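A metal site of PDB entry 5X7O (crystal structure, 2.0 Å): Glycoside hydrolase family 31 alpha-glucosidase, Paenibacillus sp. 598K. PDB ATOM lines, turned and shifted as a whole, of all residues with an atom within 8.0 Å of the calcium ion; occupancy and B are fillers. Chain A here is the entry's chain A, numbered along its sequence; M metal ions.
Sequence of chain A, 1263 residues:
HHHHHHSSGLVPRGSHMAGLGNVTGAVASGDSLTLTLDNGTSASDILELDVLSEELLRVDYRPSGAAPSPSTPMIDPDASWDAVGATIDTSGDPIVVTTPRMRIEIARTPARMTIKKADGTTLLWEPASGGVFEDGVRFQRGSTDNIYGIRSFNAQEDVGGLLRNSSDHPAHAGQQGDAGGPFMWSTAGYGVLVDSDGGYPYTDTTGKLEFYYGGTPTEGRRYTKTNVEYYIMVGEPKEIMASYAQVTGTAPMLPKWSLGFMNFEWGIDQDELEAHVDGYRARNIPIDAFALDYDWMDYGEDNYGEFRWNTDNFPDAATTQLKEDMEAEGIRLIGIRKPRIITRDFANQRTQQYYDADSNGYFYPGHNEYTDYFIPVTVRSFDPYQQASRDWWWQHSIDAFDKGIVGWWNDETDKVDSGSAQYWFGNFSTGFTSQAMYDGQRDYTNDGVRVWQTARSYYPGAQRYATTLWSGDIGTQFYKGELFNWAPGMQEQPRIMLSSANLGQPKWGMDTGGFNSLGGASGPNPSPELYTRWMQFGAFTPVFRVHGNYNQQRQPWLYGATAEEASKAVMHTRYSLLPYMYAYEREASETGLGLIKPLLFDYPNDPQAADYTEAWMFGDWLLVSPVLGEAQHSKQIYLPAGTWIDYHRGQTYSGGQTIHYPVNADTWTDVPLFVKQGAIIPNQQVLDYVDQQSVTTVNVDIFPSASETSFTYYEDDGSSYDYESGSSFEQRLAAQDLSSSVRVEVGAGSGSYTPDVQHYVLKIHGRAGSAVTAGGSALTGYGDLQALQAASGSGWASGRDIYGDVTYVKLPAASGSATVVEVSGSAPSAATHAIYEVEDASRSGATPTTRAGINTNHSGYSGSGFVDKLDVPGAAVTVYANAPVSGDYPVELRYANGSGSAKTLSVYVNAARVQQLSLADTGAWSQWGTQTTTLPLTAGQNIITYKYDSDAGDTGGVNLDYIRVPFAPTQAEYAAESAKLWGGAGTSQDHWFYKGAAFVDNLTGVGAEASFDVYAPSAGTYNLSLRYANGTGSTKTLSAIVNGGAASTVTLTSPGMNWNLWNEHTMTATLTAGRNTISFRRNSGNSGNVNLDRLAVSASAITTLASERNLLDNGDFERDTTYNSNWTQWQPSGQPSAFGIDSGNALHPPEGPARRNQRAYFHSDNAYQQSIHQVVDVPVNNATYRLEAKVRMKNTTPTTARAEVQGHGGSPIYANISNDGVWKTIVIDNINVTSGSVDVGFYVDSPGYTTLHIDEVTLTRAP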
ATOM      1  N   GLN A 786     -37.046   5.565   3.978  1.00  0.00           N
ATOM      2  CA  GLN A 786     -37.071   4.371   3.119  1.00  0.00           C
ATOM      3  C   GLN A 786     -38.475   3.725   3.093  1.00  0.00           C
ATOM      4  O   GLN A 786     -39.038   3.532   2.012  1.00  0.00           O
ATOM      5  CB  GLN A 786     -36.019   3.337   3.540  1.00  0.00           C
ATOM      6  CG  GLN A 786     -35.533   2.406   2.424  1.00  0.00           C
ATOM      7  CD  GLN A 786     -36.662   1.720   1.648  1.00  0.00           C
ATOM      8  OE1 GLN A 786     -37.160   0.666   2.054  1.00  0.00           O
ATOM      9  NE2 GLN A 786     -37.066   2.329   0.517  1.00  0.00           N
ATOM     10  N   ILE A 835     -27.986   7.260   7.035  1.00  0.00           N
ATOM     11  CA  ILE A 835     -27.827   6.089   6.156  1.00  0.00           C
ATOM     12  C   ILE A 835     -27.805   6.499   4.685  1.00  0.00           C
ATOM     13  O   ILE A 835     -28.661   7.270   4.239  1.00  0.00           O
ATOM     14  CB  ILE A 835     -28.903   5.001   6.447  1.00  0.00           C
ATOM     15  CG1 ILE A 835     -28.702   3.794   5.524  1.00  0.00           C
ATOM     16  CG2 ILE A 835     -30.326   5.529   6.313  1.00  0.00           C
ATOM     17  CD1 ILE A 835     -29.285   2.503   6.069  1.00  0.00           C
ATOM     18  N   TYR A 836     -26.814   5.989   3.945  1.00  0.00           N
ATOM     19  CA  TYR A 836     -26.723   6.194   2.497  1.00  0.00           C
ATOM     20  C   TYR A 836     -26.793   4.850   1.777  1.00  0.00           C
ATOM     21  O   TYR A 836     -25.846   4.076   1.821  1.00  0.00           O
ATOM     22  CB  TYR A 836     -25.409   6.903   2.148  1.00  0.00           C
ATOM     23  CG  TYR A 836     -25.262   8.271   2.809  1.00  0.00           C
ATOM     24  CD1 TYR A 836     -24.714   8.397   4.081  1.00  0.00           C
ATOM     25  CD2 TYR A 836     -25.702   9.424   2.162  1.00  0.00           C
ATOM     26  CE1 TYR A 836     -24.599   9.632   4.702  1.00  0.00           C
ATOM     27  CE2 TYR A 836     -25.587  10.672   2.765  1.00  0.00           C
ATOM     28  CZ  TYR A 836     -25.048  10.767   4.030  1.00  0.00           C
ATOM     29  OH  TYR A 836     -24.922  11.980   4.634  1.00  0.00           O
ATOM     30  N   GLU A 837     -27.919   4.588   1.112  1.00  0.00           N
ATOM     31  CA  GLU A 837     -28.058   3.373   0.320  1.00  0.00           C
ATOM     32  C   GLU A 837     -27.203   3.542  -0.931  1.00  0.00           C
ATOM     33  O   GLU A 837     -27.393   4.487  -1.684  1.00  0.00           O
ATOM     34  CB  GLU A 837     -29.532   3.137  -0.068  1.00  0.00           C
ATOM     35  CG  GLU A 837     -30.476   2.937   1.113  1.00  0.00           C
ATOM     36  CD  GLU A 837     -30.322   1.584   1.818  1.00  0.00           C
ATOM     37  OE1 GLU A 837     -29.672   0.662   1.291  1.00  0.00           O
ATOM     38  OE2 GLU A 837     -30.878   1.451   2.918  1.00  0.00           O
ATOM     39  N   VAL A 838     -26.228   2.639  -1.148  1.00  0.00           N
ATOM     40  CA  VAL A 838     -25.261   2.833  -2.250  1.00  0.00           C
ATOM     41  C   VAL A 838     -25.861   2.650  -3.644  1.00  0.00           C
ATOM     42  O   VAL A 838     -25.348   3.200  -4.623  1.00  0.00           O
ATOM     43  CB  VAL A 838     -23.948   2.019  -2.058  1.00  0.00           C
ATOM     44  CG1 VAL A 838     -23.199   2.549  -0.853  1.00  0.00           C
ATOM     45  CG2 VAL A 838     -24.201   0.522  -1.928  1.00  0.00           C
ATOM     46  N   GLU A 839     -26.968   1.932  -3.752  1.00  0.00           N
ATOM     47  CA  GLU A 839     -27.706   1.856  -5.021  1.00  0.00           C
ATOM     48  C   GLU A 839     -28.263   3.200  -5.505  1.00  0.00           C
ATOM     49  O   GLU A 839     -28.589   3.338  -6.681  1.00  0.00           O
ATOM     50  CB  GLU A 839     -28.843   0.825  -4.974  1.00  0.00           C
ATOM     51  CG  GLU A 839     -29.958   1.134  -3.978  1.00  0.00           C
ATOM     52  CD  GLU A 839     -29.719   0.588  -2.587  1.00  0.00           C
ATOM     53  OE1 GLU A 839     -28.534   0.413  -2.177  1.00  0.00           O
ATOM     54  OE2 GLU A 839     -30.701   0.303  -1.871  1.00  0.00           O
ATOM     55  N   ASP A 840     -28.405   4.181  -4.596  1.00  0.00           N
ATOM     56  CA  ASP A 840     -28.770   5.551  -4.963  1.00  0.00           C
ATOM     57  C   ASP A 840     -27.550   6.455  -5.209  1.00  0.00           C
ATOM     58  O   ASP A 840     -27.723   7.628  -5.573  1.00  0.00           O
ATOM     59  CB  ASP A 840     -29.629   6.200  -3.868  1.00  0.00           C
ATOM     60  CG  ASP A 840     -30.945   5.439  -3.616  1.00  0.00           C
ATOM     61  OD1 ASP A 840     -31.436   4.738  -4.522  1.00  0.00           O
ATOM     62  OD2 ASP A 840     -31.488   5.561  -2.489  1.00  0.00           O
ATOM     63  N   ASN A 855     -28.485  -4.095  -8.337  1.00  0.00           N
ATOM     64  CA  ASN A 855     -29.163  -5.388  -8.391  1.00  0.00           C
ATOM     65  C   ASN A 855     -30.033  -5.682  -7.168  1.00  0.00           C
ATOM     66  O   ASN A 855     -29.937  -5.029  -6.126  1.00  0.00           O
ATOM     67  CB  ASN A 855     -28.141  -6.514  -8.616  1.00  0.00           C
ATOM     68  CG  ASN A 855     -28.597  -7.528  -9.661  1.00  0.00           C
ATOM     69  OD1 ASN A 855     -29.780  -7.872  -9.730  1.00  0.00           O
ATOM     70  ND2 ASN A 855     -27.657  -8.002 -10.480  1.00  0.00           N
ATOM     71  N   GLY A 860     -31.855 -10.050   1.557  1.00  0.00           N
ATOM     72  CA  GLY A 860     -31.265  -9.539   2.810  1.00  0.00           C
ATOM     73  C   GLY A 860     -30.851  -8.075   2.791  1.00  0.00           C
ATOM     74  O   GLY A 860     -30.385  -7.539   3.802  1.00  0.00           O
ATOM     75  N   TYR A 861     -31.032  -7.406   1.651  1.00  0.00           N
ATOM     76  CA  TYR A 861     -30.573  -6.023   1.497  1.00  0.00           C
ATOM     77  C   TYR A 861     -31.548  -5.018   2.098  1.00  0.00           C
ATOM     78  O   TYR A 861     -32.755  -5.279   2.199  1.00  0.00           O
ATOM     79  CB  TYR A 861     -30.312  -5.682   0.025  1.00  0.00           C
ATOM     80  CG  TYR A 861     -31.518  -5.855  -0.854  1.00  0.00           C
ATOM     81  CD1 TYR A 861     -32.506  -4.873  -0.931  1.00  0.00           C
ATOM     82  CD2 TYR A 861     -31.679  -7.026  -1.612  1.00  0.00           C
ATOM     83  CE1 TYR A 861     -33.616  -5.041  -1.749  1.00  0.00           C
ATOM     84  CE2 TYR A 861     -32.785  -7.204  -2.421  1.00  0.00           C
ATOM     85  CZ  TYR A 861     -33.753  -6.227  -2.490  1.00  0.00           C
ATOM     86  OH  TYR A 861     -34.830  -6.399  -3.294  1.00  0.00           O
ATOM     87  N   SER A 862     -30.990  -3.873   2.483  1.00  0.00           N
ATOM     88  CA  SER A 862     -31.738  -2.674   2.862  1.00  0.00           C
ATOM     89  C   SER A 862     -32.090  -1.828   1.637  1.00  0.00           C
ATOM     90  O   SER A 862     -31.417  -1.862   0.601  1.00  0.00           O
ATOM     91  CB  SER A 862     -30.868  -1.846   3.818  1.00  0.00           C
ATOM     92  OG  SER A 862     -31.562  -0.716   4.335  1.00  0.00           O
ATOM     93  N   GLY A 863     -33.143  -1.048   1.748  1.00  0.00           N
ATOM     94  CA  GLY A 863     -33.567  -0.177   0.644  1.00  0.00           C
ATOM     95  C   GLY A 863     -34.066  -0.941  -0.560  1.00  0.00           C
ATOM     96  O   GLY A 863     -34.594  -2.035  -0.427  1.00  0.00           O
ATOM     97  N   SER A 864     -33.848  -0.369  -1.742  1.00  0.00           N
ATOM     98  CA  SER A 864     -34.371  -0.938  -2.977  1.00  0.00           C
ATOM     99  C   SER A 864     -33.407  -1.891  -3.655  1.00  0.00           C
ATOM    100  O   SER A 864     -33.733  -2.464  -4.699  1.00  0.00           O
ATOM    101  CB  SER A 864     -34.763   0.185  -3.938  1.00  0.00           C
ATOM    102  OG  SER A 864     -33.627   0.955  -4.309  1.00  0.00           O
ATOM    103  N   GLY A 865     -32.210  -2.073  -3.099  1.00  0.00           N
ATOM    104  CA  GLY A 865     -31.220  -2.930  -3.721  1.00  0.00           C
ATOM    105  C   GLY A 865     -29.845  -2.815  -3.111  1.00  0.00           C
ATOM    106  O   GLY A 865     -29.701  -2.430  -1.964  1.00  0.00           O
ATOM    107  N   PHE A 866     -28.846  -3.204  -3.887  1.00  0.00           N
ATOM    108  CA  PHE A 866     -27.446  -3.132  -3.500  1.00  0.00           C
ATOM    109  C   PHE A 866     -26.613  -2.911  -4.763  1.00  0.00           C
ATOM    110  O   PHE A 866     -27.160  -2.938  -5.869  1.00  0.00           O
ATOM    111  CB  PHE A 866     -27.018  -4.407  -2.795  1.00  0.00           C
ATOM    112  CG  PHE A 866     -27.278  -5.666  -3.594  1.00  0.00           C
ATOM    113  CD1 PHE A 866     -26.324  -6.166  -4.466  1.00  0.00           C
ATOM    114  CD2 PHE A 866     -28.479  -6.360  -3.434  1.00  0.00           C
ATOM    115  CE1 PHE A 866     -26.569  -7.341  -5.182  1.00  0.00           C
ATOM    116  CE2 PHE A 866     -28.728  -7.522  -4.147  1.00  0.00           C
ATOM    117  CZ  PHE A 866     -27.773  -8.005  -5.023  1.00  0.00           C
ATOM    118  N   VAL A 867     -25.318  -2.699  -4.580  1.00  0.00           N
ATOM    119  CA  VAL A 867     -24.422  -2.434  -5.695  1.00  0.00           C
ATOM    120  C   VAL A 867     -23.582  -3.674  -5.952  1.00  0.00           C
ATOM    121  O   VAL A 867     -22.984  -4.216  -5.033  1.00  0.00           O
ATOM    122  CB  VAL A 867     -23.527  -1.211  -5.399  1.00  0.00           C
ATOM    123  CG1 VAL A 867     -22.354  -1.137  -6.371  1.00  0.00           C
ATOM    124  CG2 VAL A 867     -24.371   0.062  -5.477  1.00  0.00           C
ATOM    125  N   ARG A 894     -22.063  -1.789   4.981  1.00  0.00           N
ATOM    126  CA  ARG A 894     -22.754  -3.083   4.920  1.00  0.00           C
ATOM    127  C   ARG A 894     -22.470  -3.741   3.566  1.00  0.00           C
ATOM    128  O   ARG A 894     -22.655  -3.110   2.516  1.00  0.00           O
ATOM    129  CB  ARG A 894     -24.258  -2.961   5.161  1.00  0.00           C
ATOM    130  CG  ARG A 894     -24.927  -4.323   5.391  1.00  0.00           C
ATOM    131  CD  ARG A 894     -26.315  -4.188   5.959  1.00  0.00           C
ATOM    132  NE  ARG A 894     -26.927  -5.431   6.428  1.00  0.00           N
ATOM    133  CZ  ARG A 894     -27.846  -6.166   5.779  1.00  0.00           C
ATOM    134  NH1 ARG A 894     -28.266  -5.842   4.570  1.00  0.00           N
ATOM    135  NH2 ARG A 894     -28.325  -7.261   6.368  1.00  0.00           N
ATOM    136  N   TRP A 928     -25.210 -10.875   4.960  1.00  0.00           N
ATOM    137  CA  TRP A 928     -24.553  -9.563   4.989  1.00  0.00           C
ATOM    138  C   TRP A 928     -23.802  -9.346   6.305  1.00  0.00           C
ATOM    139  O   TRP A 928     -24.193  -9.859   7.335  1.00  0.00           O
ATOM    140  CB  TRP A 928     -25.592  -8.474   4.780  1.00  0.00           C
ATOM    141  CG  TRP A 928     -26.344  -8.655   3.493  1.00  0.00           C
ATOM    142  CD1 TRP A 928     -27.383  -9.520   3.279  1.00  0.00           C
ATOM    143  CD2 TRP A 928     -26.104  -7.996   2.252  1.00  0.00           C
ATOM    144  NE1 TRP A 928     -27.812  -9.423   1.986  1.00  0.00           N
ATOM    145  CE2 TRP A 928     -27.040  -8.506   1.326  1.00  0.00           C
ATOM    146  CE3 TRP A 928     -25.184  -7.024   1.821  1.00  0.00           C
ATOM    147  CZ2 TRP A 928     -27.094  -8.070  -0.003  1.00  0.00           C
ATOM    148  CZ3 TRP A 928     -25.219  -6.614   0.489  1.00  0.00           C
ATOM    149  CH2 TRP A 928     -26.180  -7.133  -0.405  1.00  0.00           C
ATOM    150  N   LEU A 960     -22.258  -4.297  -2.076  1.00  0.00           N
ATOM    151  CA  LEU A 960     -22.338  -3.275  -1.034  1.00  0.00           C
ATOM    152  C   LEU A 960     -23.777  -2.808  -0.928  1.00  0.00           C
ATOM    153  O   LEU A 960     -24.429  -2.588  -1.936  1.00  0.00           O
ATOM    154  CB  LEU A 960     -21.435  -2.092  -1.377  1.00  0.00           C
ATOM    155  CG  LEU A 960     -19.967  -2.329  -1.713  1.00  0.00           C
ATOM    156  CD1 LEU A 960     -19.271  -0.991  -1.990  1.00  0.00           C
ATOM    157  CD2 LEU A 960     -19.235  -3.095  -0.616  1.00  0.00           C
ATOM    158  N   ASP A 961     -24.268  -2.683   0.297  1.00  0.00           N
ATOM    159  CA  ASP A 961     -25.688  -2.399   0.533  1.00  0.00           C
ATOM    160  C   ASP A 961     -25.905  -0.947   0.912  1.00  0.00           C
ATOM    161  O   ASP A 961     -26.806  -0.303   0.374  1.00  0.00           O
ATOM    162  CB  ASP A 961     -26.220  -3.300   1.653  1.00  0.00           C
ATOM    163  CG  ASP A 961     -27.736  -3.265   1.776  1.00  0.00           C
ATOM    164  OD1 ASP A 961     -28.413  -2.744   0.859  1.00  0.00           O
ATOM    165  OD2 ASP A 961     -28.261  -3.756   2.799  1.00  0.00           O
ATOM    166  N   TYR A 962     -25.120  -0.465   1.873  1.00  0.00           N
ATOM    167  CA  TYR A 962     -25.177   0.934   2.353  1.00  0.00           C
ATOM    168  C   TYR A 962     -23.967   1.305   3.192  1.00  0.00           C
ATOM    169  O   TYR A 962     -23.159   0.437   3.547  1.00  0.00           O
ATOM    170  CB  TYR A 962     -26.471   1.205   3.161  1.00  0.00           C
ATOM    171  CG  TYR A 962     -26.651   0.401   4.447  1.00  0.00           C
ATOM    172  CD1 TYR A 962     -25.876   0.653   5.587  1.00  0.00           C
ATOM    173  CD2 TYR A 962     -27.635  -0.603   4.533  1.00  0.00           C
ATOM    174  CE1 TYR A 962     -26.059  -0.060   6.758  1.00  0.00           C
ATOM    175  CE2 TYR A 962     -27.830  -1.314   5.711  1.00  0.00           C
ATOM    176  CZ  TYR A 962     -27.035  -1.043   6.809  1.00  0.00           C
ATOM    177  OH  TYR A 962     -27.214  -1.752   7.972  1.00  0.00           O
ATOM    178  N   ILE A 963     -23.846   2.605   3.485  1.00  0.00           N
ATOM    179  CA  ILE A 963     -22.962   3.055   4.551  1.00  0.00           C
ATOM    180  C   ILE A 963     -23.754   3.878   5.566  1.00  0.00           C
ATOM    181  O   ILE A 963     -24.821   4.441   5.235  1.00  0.00           O
ATOM    182  CB  ILE A 963     -21.722   3.836   4.043  1.00  0.00           C
ATOM    183  CG1 ILE A 963     -22.086   5.192   3.418  1.00  0.00           C
ATOM    184  CG2 ILE A 963     -20.913   2.990   3.062  1.00  0.00           C
ATOM    185  CD1 ILE A 963     -20.875   6.085   3.175  1.00  0.00           C
HETATM  186 CA    CA M   1     -29.240  -0.973  -0.173  1.00  0.00          CA
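Of the 22 residues printed, 5 come within 4 Å of the calcium ion.
The nearest printed residue that does not touch the calcium ion is Phe 866 (4.4 Å).
O of Asp 961 sits close to N of Val 838, at 3.4 Å.
The side-chain carboxylate (OD2) of Asp 961 lies within salt-bridge range of the guanidinium group (NH1) of Arg 894, 2.7 Å away.
N of Ser 864 sits close to OE2 of Glu 839 (3.2 Å).
The calcium ion is bound by the side-chain carboxylate (OD1) of Asp 961 (2.2 Å), the side-chain carboxylate (OE1) of Glu 837 (2.2 Å), the backbone carbonyl oxygen (O) of Gly 865 (2.4 Å), the backbone carbonyl oxygen (O) of Ser 862 (2.5 Å), the side-chain carboxylate (OE1) of Glu 839 (2.5 Å), the side-chain carboxylate (OE2) of Glu 839 (2.6 Å) and the backbone carbonyl oxygen (O) of Asp 961 (2.6 Å).
The calcium ion has seven donor atoms within binding distance.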
